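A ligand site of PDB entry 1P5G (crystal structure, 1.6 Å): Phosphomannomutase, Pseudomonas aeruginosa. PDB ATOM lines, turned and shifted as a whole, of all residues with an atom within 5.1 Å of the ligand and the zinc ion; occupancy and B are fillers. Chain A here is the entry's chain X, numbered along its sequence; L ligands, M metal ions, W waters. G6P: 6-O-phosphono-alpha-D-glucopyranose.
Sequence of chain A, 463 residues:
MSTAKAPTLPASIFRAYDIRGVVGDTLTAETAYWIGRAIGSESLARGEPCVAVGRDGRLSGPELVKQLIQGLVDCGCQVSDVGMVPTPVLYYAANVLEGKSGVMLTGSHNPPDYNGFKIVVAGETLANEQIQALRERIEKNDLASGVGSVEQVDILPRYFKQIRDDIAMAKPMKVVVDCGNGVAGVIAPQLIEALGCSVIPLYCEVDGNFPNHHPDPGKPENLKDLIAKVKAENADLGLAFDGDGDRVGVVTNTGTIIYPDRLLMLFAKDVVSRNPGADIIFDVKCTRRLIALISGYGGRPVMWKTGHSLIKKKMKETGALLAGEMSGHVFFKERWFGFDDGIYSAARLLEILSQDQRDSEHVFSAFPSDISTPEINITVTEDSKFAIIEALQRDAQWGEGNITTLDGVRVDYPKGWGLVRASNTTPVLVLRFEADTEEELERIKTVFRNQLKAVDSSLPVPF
The zinc ion is bound by the side-chain carboxylate (OD1) of Asp 246 (1.9 Å), the side-chain carboxylate (OD2) of Asp 242 (2.0 Å), O3P of SEP 108 (2.0 Å) and the side-chain carboxylate (OD2) of Asp 244 (2.0 Å).
The zinc ion has four donor atoms within binding distance.
An oxygen (O1P) of the ligand lies within salt-bridge range of the guanidinium group (NH1) of Arg 421, 2.7 Å away.
An oxygen (O4) of the ligand sits at hydrogen-bond distance from the side-chain carboxylate (OE1) of Glu 325, at 2.5 Å.
An oxygen (O1P) of the ligand is in salt-bridge range of the side-chain amino group (NZ) of Lys 285 (2.8 Å).
The side-chain hydroxyl (OH) of Tyr 17 sits at hydrogen-bond distance from an oxygen (O3P) of the ligand (2.6 Å).
An oxygen (O3P) of the ligand is in hydrogen-bond range of the backbone NH (N) of Asn 424 (2.8 Å).
The side-chain hydroxyl (OG) of Ser 327 is in hydrogen-bond range of an oxygen (O4) of the ligand (2.8 Å).
The backbone NH of His 308 lies within hydrogen-bond range of an oxygen (O3) of the ligand, at 2.8 Å.
OG1 of Thr 425 sits at hydrogen-bond distance from O2P of the ligand (2.7 Å).
O1P of SEP 108 sits at hydrogen-bond distance from an oxygen (O1) of the ligand (2.5 Å).
A ring nitrogen (NE2) of His 329 lies within hydrogen-bond range of an oxygen (O2) of the ligand, 3.0 Å away.
An oxygen (O2P) of the ligand is in hydrogen-bond range of the side-chain hydroxyl (OG) of Ser 423 (2.6 Å).
Water W2 bridges O2P of SEP 108 (2.6 Å) and O2 of the ligand (2.9 Å).
Water W5 lies within hydrogen-bond range of the side-chain carboxylate of Glu 325 (2.9 Å), the backbone NH of Ser 327 (3.2 Å) and an oxygen (O4) of the ligand (3.2 Å).
O1P of SEP 108 lies within salt-bridge range of the guanidinium group of Arg 247 (2.9 Å).
A ring nitrogen (ND1) of His 329 lies within hydrogen-bond range of the backbone carbonyl oxygen (O) of Asp 246, at 3.4 Å.
The side-chain hydroxyl (OG) of Ser 423 lies within hydrogen-bond range of the backbone NH (N) of Thr 425 (3.0 Å).
N of Gly 245 sits at hydrogen-bond distance from OD1 of Asp 242 (3.0 Å).
The side-chain carboxylate of Asp 244 lies within salt-bridge range of the side-chain amino group of Lys 118 (3.2 Å).
N of Asp 242 sits at hydrogen-bond distance from O of Arg 247.
O of Thr 306 is in hydrogen-bond range of OH of Tyr 17 (3.3 Å).
NH1 of Arg 247 lies within hydrogen-bond range of ND1 of His 109.
Merely in contact with the zinc ion: Arg 247 and Lys 118.
Within 4 Å of the zinc ion: SEP 108, Lys 118, Asp 242, Asp 244, Asp 246 and Arg 247.
The nearest printed residue that does not touch the zinc ion is His 329 (4.1 Å).
CG2 of Thr 306 touches O4 of the ligand, 3.5 Å away.
CA of Gly 307 touches O3 of the ligand, at 3.5 Å.
Hydrophobic or aromatic side chains within 4 Å of the ligand: Tyr 17, His 308 and His 329.
Within 4 Å of the ligand: Tyr 17, SEP 108, Lys 285, Thr 306, Gly 307, His 308, Glu 325, Ser 327, His 329, Arg 421, Ser 423, Asn 424 and Thr 425.
Along chain A the residues within 4 Å of the ligand span positions 17 to 425.
The nearest printed residue that does not touch the ligand is Arg 247 (4.003 Å).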
ATOM      1  N   TYR A  17       6.749 -14.643  13.064  1.00  0.00           N
ATOM      2  CA  TYR A  17       6.211 -15.311  14.254  1.00  0.00           C
ATOM      3  C   TYR A  17       4.711 -15.155  14.399  1.00  0.00           C
ATOM      4  O   TYR A  17       4.044 -15.987  15.050  1.00  0.00           O
ATOM      5  CB  TYR A  17       6.799 -14.762  15.551  1.00  0.00           C
ATOM      6  CG  TYR A  17       8.313 -14.646  15.604  1.00  0.00           C
ATOM      7  CD1 TYR A  17       9.140 -15.523  14.937  1.00  0.00           C
ATOM      8  CD2 TYR A  17       8.905 -13.639  16.351  1.00  0.00           C
ATOM      9  CE1 TYR A  17      10.522 -15.413  15.013  1.00  0.00           C
ATOM     10  CE2 TYR A  17      10.295 -13.520  16.439  1.00  0.00           C
ATOM     11  CZ  TYR A  17      11.086 -14.403  15.750  1.00  0.00           C
ATOM     12  OH  TYR A  17      12.467 -14.245  15.801  1.00  0.00           O
ATOM     13  N   SEP A 108       1.331  -7.340  22.106  1.00  0.00           N
ATOM     14  CA  SEP A 108       2.427  -7.805  22.925  1.00  0.00           C
ATOM     15  CB  SEP A 108       3.500  -8.454  22.039  1.00  0.00           C
ATOM     16  OG  SEP A 108       4.502  -8.942  22.879  1.00  0.00           O
ATOM     17  C   SEP A 108       2.961  -6.700  23.844  1.00  0.00           C
ATOM     18  O   SEP A 108       2.220  -6.227  24.707  1.00  0.00           O
ATOM     19  P   SEP A 108       5.409 -10.199  22.411  1.00  0.00           P
ATOM     20  O1P SEP A 108       6.812  -9.472  22.188  1.00  0.00           O
ATOM     21  O2P SEP A 108       4.908 -10.919  21.075  1.00  0.00           O
ATOM     22  O3P SEP A 108       5.362 -11.181  23.630  1.00  0.00           O
ATOM     23  N   HIS A 109       4.236  -6.295  23.679  1.00  0.00           N
ATOM     24  CA  HIS A 109       4.892  -5.277  24.522  1.00  0.00           C
ATOM     25  C   HIS A 109       5.094  -3.939  23.803  1.00  0.00           C
ATOM     26  O   HIS A 109       5.723  -3.004  24.365  1.00  0.00           O
ATOM     27  CB  HIS A 109       6.271  -5.768  24.944  1.00  0.00           C
ATOM     28  CG  HIS A 109       7.278  -5.761  23.818  1.00  0.00           C
ATOM     29  ND1 HIS A 109       7.658  -6.913  23.152  1.00  0.00           N
ATOM     30  CD2 HIS A 109       7.966  -4.750  23.232  1.00  0.00           C
ATOM     31  CE1 HIS A 109       8.556  -6.620  22.227  1.00  0.00           C
ATOM     32  NE2 HIS A 109       8.750  -5.311  22.245  1.00  0.00           N
ATOM     33  N   LYS A 118      -1.795 -13.556  17.149  1.00  0.00           N
ATOM     34  CA  LYS A 118      -1.052 -14.792  17.383  1.00  0.00           C
ATOM     35  C   LYS A 118      -2.027 -15.929  17.124  1.00  0.00           C
ATOM     36  O   LYS A 118      -3.159 -15.913  17.645  1.00  0.00           O
ATOM     37  CB  LYS A 118      -0.493 -14.804  18.793  1.00  0.00           C
ATOM     38  CG  LYS A 118       0.575 -13.733  18.977  1.00  0.00           C
ATOM     39  CD  LYS A 118       1.113 -13.653  20.381  1.00  0.00           C
ATOM     40  CE  LYS A 118       2.255 -12.657  20.470  1.00  0.00           C
ATOM     41  NZ  LYS A 118       2.920 -12.656  21.790  1.00  0.00           N
ATOM     42  N   ASP A 242       4.959  -8.810  30.711  1.00  0.00           N
ATOM     43  CA  ASP A 242       4.789  -7.968  29.537  1.00  0.00           C
ATOM     44  C   ASP A 242       3.293  -7.750  29.301  1.00  0.00           C
ATOM     45  O   ASP A 242       2.455  -8.259  30.056  1.00  0.00           O
ATOM     46  CB  ASP A 242       5.531  -8.523  28.308  1.00  0.00           C
ATOM     47  CG  ASP A 242       4.807  -9.617  27.592  1.00  0.00           C
ATOM     48  OD1 ASP A 242       4.034 -10.361  28.226  1.00  0.00           O
ATOM     49  OD2 ASP A 242       5.058  -9.836  26.380  1.00  0.00           O
ATOM     50  N   ASP A 244       0.939  -8.703  27.373  1.00  0.00           N
ATOM     51  CA  ASP A 244      -0.053  -9.766  27.134  1.00  0.00           C
ATOM     52  C   ASP A 244       0.137 -11.003  28.022  1.00  0.00           C
ATOM     53  O   ASP A 244      -0.635 -11.952  27.953  1.00  0.00           O
ATOM     54  CB  ASP A 244      -0.136 -10.144  25.638  1.00  0.00           C
ATOM     55  CG  ASP A 244       1.164 -10.653  25.076  1.00  0.00           C
ATOM     56  OD1 ASP A 244       1.155 -11.459  24.120  1.00  0.00           O
ATOM     57  OD2 ASP A 244       2.270 -10.265  25.511  1.00  0.00           O
ATOM     58  N   GLY A 245       1.175 -11.007  28.852  1.00  0.00           N
ATOM     59  CA  GLY A 245       1.373 -12.023  29.868  1.00  0.00           C
ATOM     60  C   GLY A 245       2.050 -13.319  29.452  1.00  0.00           C
ATOM     61  O   GLY A 245       2.053 -14.273  30.227  1.00  0.00           O
ATOM     62  N   ASP A 246       2.628 -13.354  28.250  1.00  0.00           N
ATOM     63  CA  ASP A 246       3.389 -14.527  27.843  1.00  0.00           C
ATOM     64  C   ASP A 246       4.879 -14.430  28.152  1.00  0.00           C
ATOM     65  O   ASP A 246       5.636 -15.367  27.862  1.00  0.00           O
ATOM     66  CB  ASP A 246       3.141 -14.882  26.375  1.00  0.00           C
ATOM     67  CG  ASP A 246       3.472 -13.793  25.427  1.00  0.00           C
ATOM     68  OD1 ASP A 246       4.021 -12.738  25.843  1.00  0.00           O
ATOM     69  OD2 ASP A 246       3.232 -13.911  24.214  1.00  0.00           O
ATOM     70  N   ARG A 247       5.303 -13.306  28.720  1.00  0.00           N
ATOM     71  CA  ARG A 247       6.684 -13.131  29.165  1.00  0.00           C
ATOM     72  C   ARG A 247       6.709 -12.668  30.598  1.00  0.00           C
ATOM     73  O   ARG A 247       5.838 -11.894  31.030  1.00  0.00           O
ATOM     74  CB  ARG A 247       7.400 -12.089  28.329  1.00  0.00           C
ATOM     75  CG  ARG A 247       7.611 -12.482  26.882  1.00  0.00           C
ATOM     76  CD  ARG A 247       7.869 -11.330  25.938  1.00  0.00           C
ATOM     77  NE  ARG A 247       8.343 -10.099  26.560  1.00  0.00           N
ATOM     78  CZ  ARG A 247       8.190  -8.900  26.022  1.00  0.00           C
ATOM     79  NH1 ARG A 247       7.569  -8.789  24.870  1.00  0.00           N
ATOM     80  NH2 ARG A 247       8.663  -7.806  26.614  1.00  0.00           N
ATOM     81  N   LYS A 285      20.200 -17.234  21.785  1.00  0.00           N
ATOM     82  CA  LYS A 285      20.577 -16.097  22.623  1.00  0.00           C
ATOM     83  C   LYS A 285      20.956 -16.486  24.042  1.00  0.00           C
ATOM     84  O   LYS A 285      21.360 -15.624  24.829  1.00  0.00           O
ATOM     85  CB  LYS A 285      19.445 -15.076  22.670  1.00  0.00           C
ATOM     86  CG  LYS A 285      19.116 -14.444  21.334  1.00  0.00           C
ATOM     87  CD  LYS A 285      18.035 -13.409  21.497  1.00  0.00           C
ATOM     88  CE  LYS A 285      17.599 -12.827  20.223  1.00  0.00           C
ATOM     89  NZ  LYS A 285      16.450 -11.881  20.422  1.00  0.00           N
ATOM     90  N   THR A 306      15.261 -18.364  17.836  1.00  0.00           N
ATOM     91  CA  THR A 306      14.465 -17.360  18.514  1.00  0.00           C
ATOM     92  C   THR A 306      13.062 -17.280  17.878  1.00  0.00           C
ATOM     93  O   THR A 306      12.925 -17.418  16.669  1.00  0.00           O
ATOM     94  CB  THR A 306      15.206 -15.999  18.352  1.00  0.00           C
ATOM     95  OG1 THR A 306      16.466 -16.048  19.045  1.00  0.00           O
ATOM     96  CG2 THR A 306      14.416 -14.862  18.960  1.00  0.00           C
ATOM     97  N   GLY A 307      12.039 -17.052  18.717  1.00  0.00           N
ATOM     98  CA  GLY A 307      10.694 -16.814  18.240  1.00  0.00           C
ATOM     99  C   GLY A 307       9.696 -17.781  18.834  1.00  0.00           C
ATOM    100  O   GLY A 307       9.837 -18.988  18.649  1.00  0.00           O
ATOM    101  N   HIS A 308       8.658 -17.259  19.474  1.00  0.00           N
ATOM    102  CA  HIS A 308       7.742 -18.132  20.220  1.00  0.00           C
ATOM    103  C   HIS A 308       7.148 -19.232  19.369  1.00  0.00           C
ATOM    104  O   HIS A 308       7.151 -20.401  19.761  1.00  0.00           O
ATOM    105  CB  HIS A 308       6.661 -17.292  20.951  1.00  0.00           C
ATOM    106  CG  HIS A 308       5.660 -16.664  20.046  1.00  0.00           C
ATOM    107  ND1 HIS A 308       4.483 -17.297  19.692  1.00  0.00           N
ATOM    108  CD2 HIS A 308       5.652 -15.471  19.402  1.00  0.00           C
ATOM    109  CE1 HIS A 308       3.790 -16.517  18.875  1.00  0.00           C
ATOM    110  NE2 HIS A 308       4.478 -15.405  18.689  1.00  0.00           N
ATOM    111  N   GLU A 325      13.268 -18.896  25.975  1.00  0.00           N
ATOM    112  CA  GLU A 325      14.129 -18.037  25.199  1.00  0.00           C
ATOM    113  C   GLU A 325      14.487 -16.785  25.969  1.00  0.00           C
ATOM    114  O   GLU A 325      13.774 -16.358  26.894  1.00  0.00           O
ATOM    115  CB  GLU A 325      13.477 -17.691  23.874  1.00  0.00           C
ATOM    116  CG  GLU A 325      12.154 -16.988  24.011  1.00  0.00           C
ATOM    117  CD  GLU A 325      11.633 -16.533  22.679  1.00  0.00           C
ATOM    118  OE1 GLU A 325      12.461 -16.195  21.784  1.00  0.00           O
ATOM    119  OE2 GLU A 325      10.402 -16.487  22.537  1.00  0.00           O
ATOM    120  N   SER A 327      14.193 -13.770  25.563  1.00  0.00           N
ATOM    121  CA  SER A 327      13.173 -12.719  25.705  1.00  0.00           C
ATOM    122  C   SER A 327      12.194 -12.911  26.849  1.00  0.00           C
ATOM    123  O   SER A 327      11.408 -12.020  27.118  1.00  0.00           O
ATOM    124  CB  SER A 327      12.388 -12.541  24.420  1.00  0.00           C
ATOM    125  OG  SER A 327      11.769 -13.763  24.063  1.00  0.00           O
ATOM    126  N   HIS A 329       9.973 -15.644  27.234  1.00  0.00           N
ATOM    127  CA  HIS A 329       8.943 -16.631  26.940  1.00  0.00           C
ATOM    128  C   HIS A 329       9.450 -17.966  27.477  1.00  0.00           C
ATOM    129  O   HIS A 329      10.535 -18.418  27.078  1.00  0.00           O
ATOM    130  CB  HIS A 329       8.654 -16.739  25.419  1.00  0.00           C
ATOM    131  CG  HIS A 329       8.065 -15.504  24.812  1.00  0.00           C
ATOM    132  ND1 HIS A 329       6.710 -15.350  24.612  1.00  0.00           N
ATOM    133  CD2 HIS A 329       8.645 -14.387  24.328  1.00  0.00           C
ATOM    134  CE1 HIS A 329       6.479 -14.165  24.079  1.00  0.00           C
ATOM    135  NE2 HIS A 329       7.631 -13.551  23.892  1.00  0.00           N
ATOM    136  N   GLU A 375      22.008  -7.143  25.049  1.00  0.00           N
ATOM    137  CA  GLU A 375      21.712  -7.443  23.653  1.00  0.00           C
ATOM    138  C   GLU A 375      22.079  -6.257  22.796  1.00  0.00           C
ATOM    139  O   GLU A 375      21.738  -5.118  23.112  1.00  0.00           O
ATOM    140  CB  GLU A 375      20.238  -7.775  23.488  1.00  0.00           C
ATOM    141  CG  GLU A 375      19.903  -8.553  22.239  1.00  0.00           C
ATOM    142  CD  GLU A 375      18.820  -9.588  22.466  1.00  0.00           C
ATOM    143  OE1 GLU A 375      18.856 -10.285  23.508  1.00  0.00           O
ATOM    144  OE2 GLU A 375      17.937  -9.724  21.616  1.00  0.00           O
ATOM    145  N   ARG A 421      22.508 -12.573  14.357  1.00  0.00           N
ATOM    146  CA  ARG A 421      21.347 -13.072  13.652  1.00  0.00           C
ATOM    147  C   ARG A 421      20.470 -11.895  13.270  1.00  0.00           C
ATOM    148  O   ARG A 421      20.629 -10.794  13.770  1.00  0.00           O
ATOM    149  CB  ARG A 421      20.590 -14.072  14.528  1.00  0.00           C
ATOM    150  CG  ARG A 421      20.104 -13.514  15.844  1.00  0.00           C
ATOM    151  CD  ARG A 421      19.148 -14.453  16.565  1.00  0.00           C
ATOM    152  NE  ARG A 421      17.802 -14.525  15.986  1.00  0.00           N
ATOM    153  CZ  ARG A 421      16.857 -13.606  16.137  1.00  0.00           C
ATOM    154  NH1 ARG A 421      17.092 -12.503  16.807  1.00  0.00           N
ATOM    155  NH2 ARG A 421      15.665 -13.808  15.615  1.00  0.00           N
ATOM    156  N   ALA A 422      19.571 -12.119  12.336  1.00  0.00           N
ATOM    157  CA  ALA A 422      18.617 -11.108  11.934  1.00  0.00           C
ATOM    158  C   ALA A 422      17.411 -11.176  12.858  1.00  0.00           C
ATOM    159  O   ALA A 422      16.880 -12.235  13.131  1.00  0.00           O
ATOM    160  CB  ALA A 422      18.182 -11.375  10.523  1.00  0.00           C
ATOM    161  N   SER A 423      16.977 -10.023  13.369  1.00  0.00           N
ATOM    162  CA  SER A 423      15.694  -9.922  14.037  1.00  0.00           C
ATOM    163  C   SER A 423      14.562 -10.194  13.056  1.00  0.00           C
ATOM    164  O   SER A 423      14.620  -9.785  11.890  1.00  0.00           O
ATOM    165  CB  SER A 423      15.544  -8.520  14.622  1.00  0.00           C
ATOM    166  OG  SER A 423      14.229  -8.301  15.098  1.00  0.00           O
ATOM    167  N   ASN A 424      13.523 -10.869  13.558  1.00  0.00           N
ATOM    168  CA  ASN A 424      12.298 -11.058  12.793  1.00  0.00           C
ATOM    169  C   ASN A 424      11.161 -10.113  13.239  1.00  0.00           C
ATOM    170  O   ASN A 424      10.007 -10.329  12.874  1.00  0.00           O
ATOM    171  CB  ASN A 424      11.842 -12.505  12.889  1.00  0.00           C
ATOM    172  CG  ASN A 424      12.840 -13.450  12.290  1.00  0.00           C
ATOM    173  OD1 ASN A 424      13.436 -14.315  13.003  1.00  0.00           O
ATOM    174  ND2 ASN A 424      13.052 -13.311  10.995  1.00  0.00           N
ATOM    175  N   THR A 425      11.487  -9.112  14.058  1.00  0.00           N
ATOM    176  CA  THR A 425      10.486  -8.127  14.533  1.00  0.00           C
ATOM    177  C   THR A 425      10.854  -6.691  14.231  1.00  0.00           C
ATOM    178  O   THR A 425       9.995  -5.793  14.320  1.00  0.00           O
ATOM    179  CB  THR A 425      10.246  -8.267  16.058  1.00  0.00           C
ATOM    180  OG1 THR A 425      11.421  -7.946  16.815  1.00  0.00           O
ATOM    181  CG2 THR A 425       9.886  -9.705  16.440  1.00  0.00           C
ATOM    182  N   THR A 426      12.109  -6.486  13.845  1.00  0.00           N
ATOM    183  CA  THR A 426      12.666  -5.164  13.556  1.00  0.00           C
ATOM    184  C   THR A 426      13.761  -5.284  12.483  1.00  0.00           C
ATOM    185  O   THR A 426      14.328  -6.375  12.278  1.00  0.00           O
ATOM    186  CB  THR A 426      13.277  -4.535  14.809  1.00  0.00           C
ATOM    187  OG1 THR A 426      14.337  -5.375  15.306  1.00  0.00           O
ATOM    188  CG2 THR A 426      12.265  -4.446  15.973  1.00  0.00           C
ATOM    189  N   VAL A 430      20.916  -8.634  15.462  1.00  0.00           N
ATOM    190  CA  VAL A 430      20.971  -8.857  16.906  1.00  0.00           C
ATOM    191  C   VAL A 430      22.253  -9.616  17.219  1.00  0.00           C
ATOM    192  O   VAL A 430      22.549 -10.637  16.572  1.00  0.00           O
ATOM    193  CB  VAL A 430      19.783  -9.721  17.374  1.00  0.00           C
ATOM    194  CG1 VAL A 430      19.886  -9.987  18.859  1.00  0.00           C
ATOM    195  CG2 VAL A 430      18.456  -9.096  16.992  1.00  0.00           C
HETATM  196  C1  G6P L   1       8.918 -11.231  20.304  1.00  0.00           C
HETATM  197  C2  G6P L   1       8.556 -12.701  20.274  1.00  0.00           C
HETATM  198  C3  G6P L   1       9.631 -13.515  21.005  1.00  0.00           C
HETATM  199  C4  G6P L   1      11.035 -13.163  20.453  1.00  0.00           C
HETATM  200  C5  G6P L   1      11.261 -11.632  20.456  1.00  0.00           C
HETATM  201  C6  G6P L   1      12.594 -11.247  19.821  1.00  0.00           C
HETATM  202  O1  G6P L   1       8.906 -10.778  21.664  1.00  0.00           O
HETATM  203  O2  G6P L   1       7.276 -12.935  20.946  1.00  0.00           O
HETATM  204  O3  G6P L   1       9.299 -14.875  20.845  1.00  0.00           O
HETATM  205  O4  G6P L   1      11.978 -13.775  21.272  1.00  0.00           O
HETATM  206  O5  G6P L   1      10.243 -10.994  19.721  1.00  0.00           O
HETATM  207  O6  G6P L   1      12.543 -11.639  18.423  1.00  0.00           O
HETATM  208  P   G6P L   1      13.689 -11.095  17.469  1.00  0.00           P
HETATM  209  O1P G6P L   1      15.032 -11.294  18.112  1.00  0.00           O
HETATM  210  O2P G6P L   1      13.452  -9.633  17.220  1.00  0.00           O
HETATM  211  O3P G6P L   1      13.516 -11.891  16.198  1.00  0.00           O
HETATM  212 ZN    ZN M   1       4.089 -10.958  25.113  1.00  0.00          ZN
HETATM  213  O   HOH W   1      14.538  -7.874  19.093  1.00  0.00           O
HETATM  214  O   HOH W   2       5.739 -11.760  18.760  1.00  0.00           O
HETATM  215  O   HOH W   3       6.889  -8.672  19.576  1.00  0.00           O
HETATM  216  O   HOH W   4      11.299  -9.003  22.998  1.00  0.00           O
HETATM  217  O   HOH W   5      14.737 -14.665  22.583  1.00  0.00           O
